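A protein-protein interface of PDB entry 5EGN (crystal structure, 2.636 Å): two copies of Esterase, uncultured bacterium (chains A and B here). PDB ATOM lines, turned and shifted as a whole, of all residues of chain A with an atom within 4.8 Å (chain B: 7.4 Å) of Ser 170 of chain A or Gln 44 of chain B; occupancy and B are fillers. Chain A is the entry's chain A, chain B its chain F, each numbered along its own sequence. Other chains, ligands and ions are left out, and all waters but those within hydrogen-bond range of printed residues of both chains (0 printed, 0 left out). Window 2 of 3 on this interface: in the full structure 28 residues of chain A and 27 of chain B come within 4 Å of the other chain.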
ATOM      1  N   ILE A 139     -26.177  30.735  -8.725  1.00  0.00           N
ATOM      2  CA  ILE A 139     -24.956  30.675  -7.928  1.00  0.00           C
ATOM      3  C   ILE A 139     -24.285  32.044  -7.808  1.00  0.00           C
ATOM      4  O   ILE A 139     -23.806  32.424  -6.734  1.00  0.00           O
ATOM      5  CB  ILE A 139     -23.971  29.657  -8.532  1.00  0.00           C
ATOM      6  CG1 ILE A 139     -24.550  28.242  -8.430  1.00  0.00           C
ATOM      7  CG2 ILE A 139     -22.620  29.719  -7.836  1.00  0.00           C
ATOM      8  CD1 ILE A 139     -23.854  27.222  -9.300  1.00  0.00           C
ATOM      9  N   LYS A 166     -20.315  29.839   0.918  1.00  0.00           N
ATOM     10  CA  LYS A 166     -20.392  29.750  -0.535  1.00  0.00           C
ATOM     11  C   LYS A 166     -20.357  28.293  -0.973  1.00  0.00           C
ATOM     12  O   LYS A 166     -20.898  27.932  -2.019  1.00  0.00           O
ATOM     13  CB  LYS A 166     -19.255  30.532  -1.197  1.00  0.00           C
ATOM     14  CG  LYS A 166     -19.579  31.996  -1.444  1.00  0.00           C
ATOM     15  CD  LYS A 166     -18.513  32.665  -2.299  1.00  0.00           C
ATOM     16  CE  LYS A 166     -18.845  34.129  -2.548  1.00  0.00           C
ATOM     17  NZ  LYS A 166     -17.825  34.799  -3.403  1.00  0.00           N
ATOM     18  N   ALA A 167     -19.719  27.458  -0.160  1.00  0.00           N
ATOM     19  CA  ALA A 167     -19.649  26.030  -0.435  1.00  0.00           C
ATOM     20  C   ALA A 167     -20.979  25.336  -0.153  1.00  0.00           C
ATOM     21  O   ALA A 167     -21.347  24.385  -0.843  1.00  0.00           O
ATOM     22  CB  ALA A 167     -18.545  25.396   0.384  1.00  0.00           C
ATOM     23  N   HIS A 168     -21.694  25.819   0.860  1.00  0.00           N
ATOM     24  CA  HIS A 168     -22.947  25.198   1.290  1.00  0.00           C
ATOM     25  C   HIS A 168     -23.992  25.060   0.180  1.00  0.00           C
ATOM     26  O   HIS A 168     -24.622  24.010   0.049  1.00  0.00           O
ATOM     27  CB  HIS A 168     -23.552  25.983   2.456  1.00  0.00           C
ATOM     28  CG  HIS A 168     -23.166  25.459   3.804  1.00  0.00           C
ATOM     29  ND1 HIS A 168     -23.480  24.185   4.224  1.00  0.00           N
ATOM     30  CD2 HIS A 168     -22.503  26.040   4.832  1.00  0.00           C
ATOM     31  CE1 HIS A 168     -23.022  24.001   5.450  1.00  0.00           C
ATOM     32  NE2 HIS A 168     -22.426  25.112   5.841  1.00  0.00           N
ATOM     33  N   PHE A 169     -24.185  26.108  -0.618  1.00  0.00           N
ATOM     34  CA  PHE A 169     -25.224  26.070  -1.644  1.00  0.00           C
ATOM     35  C   PHE A 169     -24.702  25.563  -2.986  1.00  0.00           C
ATOM     36  O   PHE A 169     -25.472  25.390  -3.930  1.00  0.00           O
ATOM     37  CB  PHE A 169     -25.866  27.452  -1.822  1.00  0.00           C
ATOM     38  CG  PHE A 169     -24.936  28.501  -2.373  1.00  0.00           C
ATOM     39  CD1 PHE A 169     -24.766  28.647  -3.741  1.00  0.00           C
ATOM     40  CD2 PHE A 169     -24.264  29.363  -1.526  1.00  0.00           C
ATOM     41  CE1 PHE A 169     -23.924  29.613  -4.250  1.00  0.00           C
ATOM     42  CE2 PHE A 169     -23.425  30.335  -2.033  1.00  0.00           C
ATOM     43  CZ  PHE A 169     -23.253  30.458  -3.395  1.00  0.00           C
ATOM     44  N   SER A 170     -23.397  25.330  -3.068  1.00  0.00           N
ATOM     45  CA  SER A 170     -22.795  24.822  -4.295  1.00  0.00           C
ATOM     46  C   SER A 170     -22.682  23.304  -4.253  1.00  0.00           C
ATOM     47  O   SER A 170     -22.335  22.670  -5.250  1.00  0.00           O
ATOM     48  CB  SER A 170     -21.418  25.450  -4.519  1.00  0.00           C
ATOM     49  OG  SER A 170     -21.521  26.853  -4.690  1.00  0.00           O
ATOM     50  N   VAL A 171     -22.977  22.725  -3.095  1.00  0.00           N
ATOM     51  CA  VAL A 171     -22.953  21.276  -2.939  1.00  0.00           C
ATOM     52  C   VAL A 171     -24.374  20.717  -2.936  1.00  0.00           C
ATOM     53  O   VAL A 171     -25.111  20.889  -1.964  1.00  0.00           O
ATOM     54  CB  VAL A 171     -22.227  20.857  -1.645  1.00  0.00           C
ATOM     55  CG1 VAL A 171     -22.282  19.348  -1.467  1.00  0.00           C
ATOM     56  CG2 VAL A 171     -20.786  21.341  -1.669  1.00  0.00           C
ATOM     57  N   PRO A 172     -24.763  20.049  -4.035  1.00  0.00           N
ATOM     58  CA  PRO A 172     -26.107  19.482  -4.198  1.00  0.00           C
ATOM     59  C   PRO A 172     -26.432  18.454  -3.122  1.00  0.00           C
ATOM     60  O   PRO A 172     -27.601  18.238  -2.803  1.00  0.00           O
ATOM     61  CB  PRO A 172     -26.045  18.818  -5.579  1.00  0.00           C
ATOM     62  CG  PRO A 172     -24.932  19.506  -6.285  1.00  0.00           C
ATOM     63  CD  PRO A 172     -23.925  19.821  -5.225  1.00  0.00           C
ATOM     64  N   TYR B  16     -20.305  13.680   1.133  1.00  0.00           N
ATOM     65  CA  TYR B  16     -20.713  14.746   0.223  1.00  0.00           C
ATOM     66  C   TYR B  16     -19.886  14.751  -1.065  1.00  0.00           C
ATOM     67  O   TYR B  16     -18.728  14.354  -1.068  1.00  0.00           O
ATOM     68  CB  TYR B  16     -20.600  16.112   0.913  1.00  0.00           C
ATOM     69  CG  TYR B  16     -21.501  16.302   2.118  1.00  0.00           C
ATOM     70  CD1 TYR B  16     -22.843  16.627   1.964  1.00  0.00           C
ATOM     71  CD2 TYR B  16     -21.002  16.183   3.410  1.00  0.00           C
ATOM     72  CE1 TYR B  16     -23.667  16.813   3.062  1.00  0.00           C
ATOM     73  CE2 TYR B  16     -21.820  16.369   4.514  1.00  0.00           C
ATOM     74  CZ  TYR B  16     -23.151  16.683   4.334  1.00  0.00           C
ATOM     75  OH  TYR B  16     -23.967  16.868   5.429  1.00  0.00           O
ATOM     76  N   GLY B  17     -20.495  15.199  -2.159  1.00  0.00           N
ATOM     77  CA  GLY B  17     -19.766  15.485  -3.385  1.00  0.00           C
ATOM     78  C   GLY B  17     -19.389  14.327  -4.296  1.00  0.00           C
ATOM     79  O   GLY B  17     -19.747  13.175  -4.053  1.00  0.00           O
ATOM     80  N   GLU B  18     -18.654  14.659  -5.356  1.00  0.00           N
ATOM     81  CA  GLU B  18     -18.190  13.689  -6.348  1.00  0.00           C
ATOM     82  C   GLU B  18     -16.703  13.860  -6.656  1.00  0.00           C
ATOM     83  O   GLU B  18     -16.172  14.966  -6.575  1.00  0.00           O
ATOM     84  CB  GLU B  18     -18.980  13.825  -7.649  1.00  0.00           C
ATOM     85  CG  GLU B  18     -20.425  13.391  -7.580  1.00  0.00           C
ATOM     86  CD  GLU B  18     -21.120  13.546  -8.918  1.00  0.00           C
ATOM     87  OE1 GLU B  18     -20.573  14.252  -9.792  1.00  0.00           O
ATOM     88  OE2 GLU B  18     -22.208  12.962  -9.099  1.00  0.00           O
ATOM     89  N   GLN B  38     -13.650  22.530   6.357  1.00  0.00           N
ATOM     90  CA  GLN B  38     -12.959  21.801   5.296  1.00  0.00           C
ATOM     91  C   GLN B  38     -13.936  20.976   4.471  1.00  0.00           C
ATOM     92  O   GLN B  38     -13.825  20.901   3.246  1.00  0.00           O
ATOM     93  CB  GLN B  38     -11.880  20.883   5.879  1.00  0.00           C
ATOM     94  CG  GLN B  38     -10.613  21.592   6.312  1.00  0.00           C
ATOM     95  CD  GLN B  38     -10.797  22.411   7.571  1.00  0.00           C
ATOM     96  OE1 GLN B  38     -11.366  21.937   8.555  1.00  0.00           O
ATOM     97  NE2 GLN B  38     -10.318  23.649   7.547  1.00  0.00           N
ATOM     98  N   THR B  39     -14.892  20.370   5.165  1.00  0.00           N
ATOM     99  CA  THR B  39     -15.814  19.399   4.582  1.00  0.00           C
ATOM    100  C   THR B  39     -16.517  19.880   3.316  1.00  0.00           C
ATOM    101  O   THR B  39     -16.535  19.177   2.306  1.00  0.00           O
ATOM    102  CB  THR B  39     -16.892  18.994   5.605  1.00  0.00           C
ATOM    103  OG1 THR B  39     -16.270  18.378   6.739  1.00  0.00           O
ATOM    104  CG2 THR B  39     -17.881  18.020   4.984  1.00  0.00           C
ATOM    105  N   PHE B  40     -17.086  21.078   3.368  1.00  0.00           N
ATOM    106  CA  PHE B  40     -17.943  21.554   2.286  1.00  0.00           C
ATOM    107  C   PHE B  40     -17.222  22.320   1.168  1.00  0.00           C
ATOM    108  O   PHE B  40     -17.620  22.208   0.007  1.00  0.00           O
ATOM    109  CB  PHE B  40     -19.071  22.407   2.870  1.00  0.00           C
ATOM    110  CG  PHE B  40     -19.996  21.634   3.764  1.00  0.00           C
ATOM    111  CD1 PHE B  40     -21.027  20.880   3.227  1.00  0.00           C
ATOM    112  CD2 PHE B  40     -19.822  21.639   5.138  1.00  0.00           C
ATOM    113  CE1 PHE B  40     -21.874  20.159   4.044  1.00  0.00           C
ATOM    114  CE2 PHE B  40     -20.665  20.920   5.960  1.00  0.00           C
ATOM    115  CZ  PHE B  40     -21.692  20.179   5.412  1.00  0.00           C
ATOM    116  N   PRO B  41     -16.184  23.112   1.497  1.00  0.00           N
ATOM    117  CA  PRO B  41     -15.397  23.639   0.375  1.00  0.00           C
ATOM    118  C   PRO B  41     -14.766  22.537  -0.476  1.00  0.00           C
ATOM    119  O   PRO B  41     -14.692  22.676  -1.696  1.00  0.00           O
ATOM    120  CB  PRO B  41     -14.322  24.476   1.072  1.00  0.00           C
ATOM    121  CG  PRO B  41     -14.990  24.951   2.309  1.00  0.00           C
ATOM    122  CD  PRO B  41     -15.861  23.807   2.758  1.00  0.00           C
ATOM    123  N   PHE B  42     -14.331  21.456   0.161  1.00  0.00           N
ATOM    124  CA  PHE B  42     -13.736  20.339  -0.562  1.00  0.00           C
ATOM    125  C   PHE B  42     -14.797  19.419  -1.157  1.00  0.00           C
ATOM    126  O   PHE B  42     -14.491  18.569  -1.992  1.00  0.00           O
ATOM    127  CB  PHE B  42     -12.802  19.543   0.352  1.00  0.00           C
ATOM    128  CG  PHE B  42     -11.446  20.164   0.512  1.00  0.00           C
ATOM    129  CD1 PHE B  42     -10.450  19.927  -0.419  1.00  0.00           C
ATOM    130  CD2 PHE B  42     -11.170  20.992   1.587  1.00  0.00           C
ATOM    131  CE1 PHE B  42      -9.202  20.500  -0.278  1.00  0.00           C
ATOM    132  CE2 PHE B  42      -9.925  21.566   1.733  1.00  0.00           C
ATOM    133  CZ  PHE B  42      -8.941  21.323   0.798  1.00  0.00           C
ATOM    134  N   ALA B  43     -16.043  19.593  -0.729  1.00  0.00           N
ATOM    135  CA  ALA B  43     -17.148  18.831  -1.297  1.00  0.00           C
ATOM    136  C   ALA B  43     -17.524  19.388  -2.666  1.00  0.00           C
ATOM    137  O   ALA B  43     -18.255  18.755  -3.426  1.00  0.00           O
ATOM    138  CB  ALA B  43     -18.347  18.849  -0.366  1.00  0.00           C
ATOM    139  N   GLN B  44     -17.015  20.577  -2.972  1.00  0.00           N
ATOM    140  CA  GLN B  44     -17.238  21.198  -4.273  1.00  0.00           C
ATOM    141  C   GLN B  44     -16.422  20.506  -5.358  1.00  0.00           C
ATOM    142  O   GLN B  44     -16.849  20.423  -6.509  1.00  0.00           O
ATOM    143  CB  GLN B  44     -16.881  22.686  -4.235  1.00  0.00           C
ATOM    144  CG  GLN B  44     -17.631  23.498  -3.193  1.00  0.00           C
ATOM    145  CD  GLN B  44     -17.217  24.958  -3.193  1.00  0.00           C
ATOM    146  OE1 GLN B  44     -16.361  25.372  -2.412  1.00  0.00           O
ATOM    147  NE2 GLN B  44     -17.825  25.745  -4.072  1.00  0.00           N
ATOM    148  N   THR B  45     -15.246  20.011  -4.984  1.00  0.00           N
ATOM    149  CA  THR B  45     -14.296  19.480  -5.955  1.00  0.00           C
ATOM    150  C   THR B  45     -14.014  17.993  -5.769  1.00  0.00           C
ATOM    151  O   THR B  45     -13.515  17.332  -6.680  1.00  0.00           O
ATOM    152  CB  THR B  45     -12.960  20.243  -5.889  1.00  0.00           C
ATOM    153  OG1 THR B  45     -12.441  20.184  -4.555  1.00  0.00           O
ATOM    154  CG2 THR B  45     -13.157  21.696  -6.284  1.00  0.00           C
ATOM    155  N   ASN B  46     -14.331  17.468  -4.590  1.00  0.00           N
ATOM    156  CA  ASN B  46     -13.995  16.088  -4.259  1.00  0.00           C
ATOM    157  C   ASN B  46     -15.134  15.329  -3.597  1.00  0.00           C
ATOM    158  O   ASN B  46     -16.135  15.919  -3.196  1.00  0.00           O
ATOM    159  CB  ASN B  46     -12.771  16.054  -3.342  1.00  0.00           C
ATOM    160  CG  ASN B  46     -11.546  16.667  -3.981  1.00  0.00           C
ATOM    161  OD1 ASN B  46     -11.366  17.885  -3.967  1.00  0.00           O
ATOM    162  ND2 ASN B  46     -10.687  15.823  -4.540  1.00  0.00           N
ATOM    163  N   HIS B  47     -14.969  14.016  -3.481  1.00  0.00           N
ATOM    164  CA  HIS B  47     -15.887  13.198  -2.701  1.00  0.00           C
ATOM    165  C   HIS B  47     -15.408  13.138  -1.256  1.00  0.00           C
ATOM    166  O   HIS B  47     -14.566  12.317  -0.897  1.00  0.00           O
ATOM    167  CB  HIS B  47     -16.003  11.789  -3.283  1.00  0.00           C
ATOM    168  CG  HIS B  47     -16.970  10.912  -2.548  1.00  0.00           C
ATOM    169  ND1 HIS B  47     -17.018   9.545  -2.726  1.00  0.00           N
ATOM    170  CD2 HIS B  47     -17.929  11.205  -1.640  1.00  0.00           C
ATOM    171  CE1 HIS B  47     -17.961   9.036  -1.954  1.00  0.00           C
ATOM    172  NE2 HIS B  47     -18.530  10.022  -1.284  1.00  0.00           N
ATOM    173  N   VAL B  48     -15.955  14.024  -0.432  1.00  0.00           N
ATOM    174  CA  VAL B  48     -15.589  14.116   0.972  1.00  0.00           C
ATOM    175  C   VAL B  48     -16.326  13.091   1.831  1.00  0.00           C
ATOM    176  O   VAL B  48     -17.553  12.990   1.787  1.00  0.00           O
ATOM    177  CB  VAL B  48     -15.873  15.526   1.523  1.00  0.00           C
ATOM    178  CG1 VAL B  48     -15.660  15.567   3.027  1.00  0.00           C
ATOM    179  CG2 VAL B  48     -15.000  16.552   0.822  1.00  0.00           C
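Ser 170 of chain A touches just one residue of chain B: Gln 44.
Of chain A, only Ala 167 (3.5 Å) and Ser 170 (3.6 Å) come within 4 Å of Gln 44 of chain B.
Printed residues of chain A within 4 Å of Phe 40 of chain B: Ala 167 (3.3 Å), His 168 (3.9 Å) and Val 171 (3.7 Å).
Printed residues of chain B within 4 Å of Val 171 of chain A: Phe 40 and Ala 43.
Of the printed residues of chain B, Ala 167 of chain A touches Phe 40 (3.3 Å), Pro 41 (3.5 Å) and Gln 44 (3.5 Å).
Of the printed residues of chain A, Ala 43 of chain B touches Val 171.
The nearest residue of chain B that does not touch Ser 170 of chain A is Ala 43 of chain B (5.9 Å).
No position is printed for both chains.
Of the 7 pairs that touch across the chains among the printed residues, none has its exchanged pair printed and touching as well.
The backbone carbonyl oxygen of Lys 166 of chain A is in hydrogen-bond range of the side-chain hydroxyl of Ser 170 of chain A (2.9 Å).
The backbone carbonyl oxygen of Pro 41 of chain B sits close to the side-chain amide oxygen of Gln 44 of chain B (3.3 Å).
Of the 14 printed residues of chain B, 4 touch a printed residue of chain A.
Hydrophobic or aromatic side chains of chain B within 4 Å of the printed part of chain A: Phe 40, Pro 41 and Ala 43.
Hydrophobic or aromatic side chains of chain A within 4 Å of the printed part of chain B: Ala 167, His 168 and Val 171.
Among the printed residues, no Asp or Glu carboxylate lies within 4 Å of a Lys or Arg side-chain nitrogen of the other chain.
Among the printed residues, pairs that only touch across the chains: Ala 167 of chain A with Phe 40 of chain B, Ala 167 of chain A with Pro 41 of chain B, Ala 167 of chain A with Gln 44 of chain B, His 168 of chain A with Phe 40 of chain B, Ser 170 of chain A with Gln 44 of chain B, Val 171 of chain A with Phe 40 of chain B and Val 171 of chain A with Ala 43 of chain B.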
